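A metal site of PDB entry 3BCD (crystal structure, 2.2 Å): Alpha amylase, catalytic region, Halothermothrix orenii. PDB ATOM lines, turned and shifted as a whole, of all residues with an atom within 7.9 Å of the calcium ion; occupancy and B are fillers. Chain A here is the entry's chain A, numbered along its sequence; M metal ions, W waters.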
ATOM      1  N   SER A 410      16.164  -7.794 -21.863  1.00  0.00           N
ATOM      2  CA  SER A 410      17.173  -7.224 -22.720  1.00  0.00           C
ATOM      3  C   SER A 410      16.728  -5.777 -23.110  1.00  0.00           C
ATOM      4  O   SER A 410      17.591  -4.858 -23.215  1.00  0.00           O
ATOM      5  CB  SER A 410      17.517  -8.209 -23.918  1.00  0.00           C
ATOM      6  OG  SER A 410      16.912  -7.847 -25.155  1.00  0.00           O
ATOM      7  N   PHE A 411      15.431  -5.504 -23.213  1.00  0.00           N
ATOM      8  CA  PHE A 411      14.988  -4.102 -23.527  1.00  0.00           C
ATOM      9  C   PHE A 411      15.212  -3.249 -22.275  1.00  0.00           C
ATOM     10  O   PHE A 411      15.628  -2.087 -22.400  1.00  0.00           O
ATOM     11  CB  PHE A 411      13.534  -3.961 -23.913  1.00  0.00           C
ATOM     12  CG  PHE A 411      13.225  -2.627 -24.635  1.00  0.00           C
ATOM     13  CD1 PHE A 411      13.264  -2.544 -26.034  1.00  0.00           C
ATOM     14  CD2 PHE A 411      12.922  -1.504 -23.957  1.00  0.00           C
ATOM     15  CE1 PHE A 411      13.000  -1.310 -26.708  1.00  0.00           C
ATOM     16  CE2 PHE A 411      12.651  -0.248 -24.650  1.00  0.00           C
ATOM     17  CZ  PHE A 411      12.673  -0.186 -25.974  1.00  0.00           C
ATOM     18  N   PHE A 412      14.998  -3.851 -21.084  1.00  0.00           N
ATOM     19  CA  PHE A 412      15.185  -3.091 -19.897  1.00  0.00           C
ATOM     20  C   PHE A 412      16.671  -2.790 -19.737  1.00  0.00           C
ATOM     21  O   PHE A 412      16.974  -1.778 -19.220  1.00  0.00           O
ATOM     22  CB  PHE A 412      14.576  -3.698 -18.626  1.00  0.00           C
ATOM     23  CG  PHE A 412      13.140  -4.061 -18.714  1.00  0.00           C
ATOM     24  CD1 PHE A 412      12.689  -5.236 -18.135  1.00  0.00           C
ATOM     25  CD2 PHE A 412      12.223  -3.262 -19.362  1.00  0.00           C
ATOM     26  CE1 PHE A 412      11.363  -5.630 -18.198  1.00  0.00           C
ATOM     27  CE2 PHE A 412      10.832  -3.655 -19.419  1.00  0.00           C
ATOM     28  CZ  PHE A 412      10.426  -4.847 -18.857  1.00  0.00           C
ATOM     29  N   VAL A 413      17.592  -3.688 -20.104  1.00  0.00           N
ATOM     30  CA  VAL A 413      19.059  -3.366 -20.148  1.00  0.00           C
ATOM     31  C   VAL A 413      19.405  -2.206 -21.127  1.00  0.00           C
ATOM     32  O   VAL A 413      20.271  -1.374 -20.856  1.00  0.00           O
ATOM     33  CB  VAL A 413      19.907  -4.625 -20.572  1.00  0.00           C
ATOM     34  CG1 VAL A 413      21.414  -4.266 -20.665  1.00  0.00           C
ATOM     35  CG2 VAL A 413      19.670  -5.884 -19.623  1.00  0.00           C
ATOM     36  N   ASP A 414      18.730  -2.201 -22.277  1.00  0.00           N
ATOM     37  CA  ASP A 414      18.811  -1.126 -23.302  1.00  0.00           C
ATOM     38  C   ASP A 414      18.471   0.155 -22.611  1.00  0.00           C
ATOM     39  O   ASP A 414      19.203   1.138 -22.699  1.00  0.00           O
ATOM     40  CB  ASP A 414      17.861  -1.445 -24.523  1.00  0.00           C
ATOM     41  CG  ASP A 414      17.996  -0.493 -25.743  1.00  0.00           C
ATOM     42  OD1 ASP A 414      18.811   0.432 -25.772  1.00  0.00           O
ATOM     43  OD2 ASP A 414      17.226  -0.672 -26.714  1.00  0.00           O
ATOM     44  N   MET A 415      17.338   0.183 -21.913  1.00  0.00           N
ATOM     45  CA  MET A 415      16.921   1.427 -21.245  1.00  0.00           C
ATOM     46  C   MET A 415      17.958   2.027 -20.275  1.00  0.00           C
ATOM     47  O   MET A 415      17.843   3.140 -19.939  1.00  0.00           O
ATOM     48  CB  MET A 415      15.626   1.237 -20.481  1.00  0.00           C
ATOM     49  CG  MET A 415      14.400   1.114 -21.369  1.00  0.00           C
ATOM     50  SD  MET A 415      12.856   0.581 -20.609  1.00  0.00           S
ATOM     51  CE  MET A 415      12.677   1.799 -19.333  1.00  0.00           C
ATOM     52  N   LEU A 416      18.934   1.285 -19.772  1.00  0.00           N
ATOM     53  CA  LEU A 416      19.832   1.835 -18.733  1.00  0.00           C
ATOM     54  C   LEU A 416      20.443   3.161 -19.232  1.00  0.00           C
ATOM     55  O   LEU A 416      20.583   4.089 -18.457  1.00  0.00           O
ATOM     56  CB  LEU A 416      20.919   0.845 -18.368  1.00  0.00           C
ATOM     57  CG  LEU A 416      20.474  -0.465 -17.728  1.00  0.00           C
ATOM     58  CD1 LEU A 416      21.655  -1.480 -17.622  1.00  0.00           C
ATOM     59  CD2 LEU A 416      19.864  -0.172 -16.342  1.00  0.00           C
ATOM     60  N   ASN A 417      20.735   3.266 -20.529  1.00  0.00           N
ATOM     61  CA  ASN A 417      21.377   4.466 -21.059  1.00  0.00           C
ATOM     62  C   ASN A 417      20.527   5.109 -22.152  1.00  0.00           C
ATOM     63  O   ASN A 417      21.017   5.908 -22.906  1.00  0.00           O
ATOM     64  CB  ASN A 417      22.795   4.166 -21.554  1.00  0.00           C
ATOM     65  CG  ASN A 417      22.795   3.272 -22.754  1.00  0.00           C
ATOM     66  OD1 ASN A 417      21.754   2.865 -23.216  1.00  0.00           O
ATOM     67  ND2 ASN A 417      23.954   2.967 -23.261  1.00  0.00           N
ATOM     68  N   GLY A 418      19.260   4.746 -22.239  1.00  0.00           N
ATOM     69  CA  GLY A 418      18.427   5.332 -23.246  1.00  0.00           C
ATOM     70  C   GLY A 418      18.140   4.320 -24.324  1.00  0.00           C
ATOM     71  O   GLY A 418      19.101   3.729 -24.914  1.00  0.00           O
ATOM     72  N   ALA A 419      16.822   4.093 -24.513  1.00  0.00           N
ATOM     73  CA  ALA A 419      16.242   3.232 -25.540  1.00  0.00           C
ATOM     74  C   ALA A 419      15.273   3.999 -26.433  1.00  0.00           C
ATOM     75  O   ALA A 419      14.880   5.134 -26.147  1.00  0.00           O
ATOM     76  CB  ALA A 419      15.511   2.043 -24.890  1.00  0.00           C
ATOM     77  N   TYR A 420      14.835   3.369 -27.492  1.00  0.00           N
ATOM     78  CA  TYR A 420      13.794   3.912 -28.308  1.00  0.00           C
ATOM     79  C   TYR A 420      12.454   3.427 -27.825  1.00  0.00           C
ATOM     80  O   TYR A 420      12.022   2.286 -28.130  1.00  0.00           O
ATOM     81  CB  TYR A 420      14.019   3.518 -29.768  1.00  0.00           C
ATOM     82  CG  TYR A 420      13.288   4.436 -30.661  1.00  0.00           C
ATOM     83  CD1 TYR A 420      13.833   5.615 -31.013  1.00  0.00           C
ATOM     84  CD2 TYR A 420      12.002   4.142 -31.086  1.00  0.00           C
ATOM     85  CE1 TYR A 420      13.176   6.445 -31.805  1.00  0.00           C
ATOM     86  CE2 TYR A 420      11.315   4.978 -31.886  1.00  0.00           C
ATOM     87  CZ  TYR A 420      11.899   6.140 -32.248  1.00  0.00           C
ATOM     88  OH  TYR A 420      11.212   6.997 -33.061  1.00  0.00           O
ATOM     89  N   ASP A 541      11.886   7.373 -20.740  1.00  0.00           N
ATOM     90  CA  ASP A 541      13.353   7.396 -20.416  1.00  0.00           C
ATOM     91  C   ASP A 541      13.950   8.797 -20.465  1.00  0.00           C
ATOM     92  O   ASP A 541      15.157   8.958 -20.403  1.00  0.00           O
ATOM     93  CB  ASP A 541      14.187   6.390 -21.238  1.00  0.00           C
ATOM     94  CG  ASP A 541      14.292   6.729 -22.731  1.00  0.00           C
ATOM     95  OD1 ASP A 541      15.052   6.046 -23.432  1.00  0.00           O
ATOM     96  OD2 ASP A 541      13.654   7.666 -23.244  1.00  0.00           O
HETATM   97 CA    CA M   1      20.339   1.741 -24.643  1.00  0.00          CA
HETATM   98  O   HOH W   1      22.294  -0.165 -24.476  1.00  0.00           O
HETATM   99  O   HOH W   2      21.463   2.529 -26.549  1.00  0.00           O
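Of the 12 residues printed, 3 come within 4 Å of the calcium ion.
The calcium ion is bound by OD1 of Asn 417 (2.3 Å), OD1 of Asp 414 (2.3 Å), O of Asp 414 (2.3 Å), water W2 (2.3 Å), O of Gly 418 (2.4 Å) and water W1 (2.7 Å).
The calcium ion has six donor atoms within binding distance.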
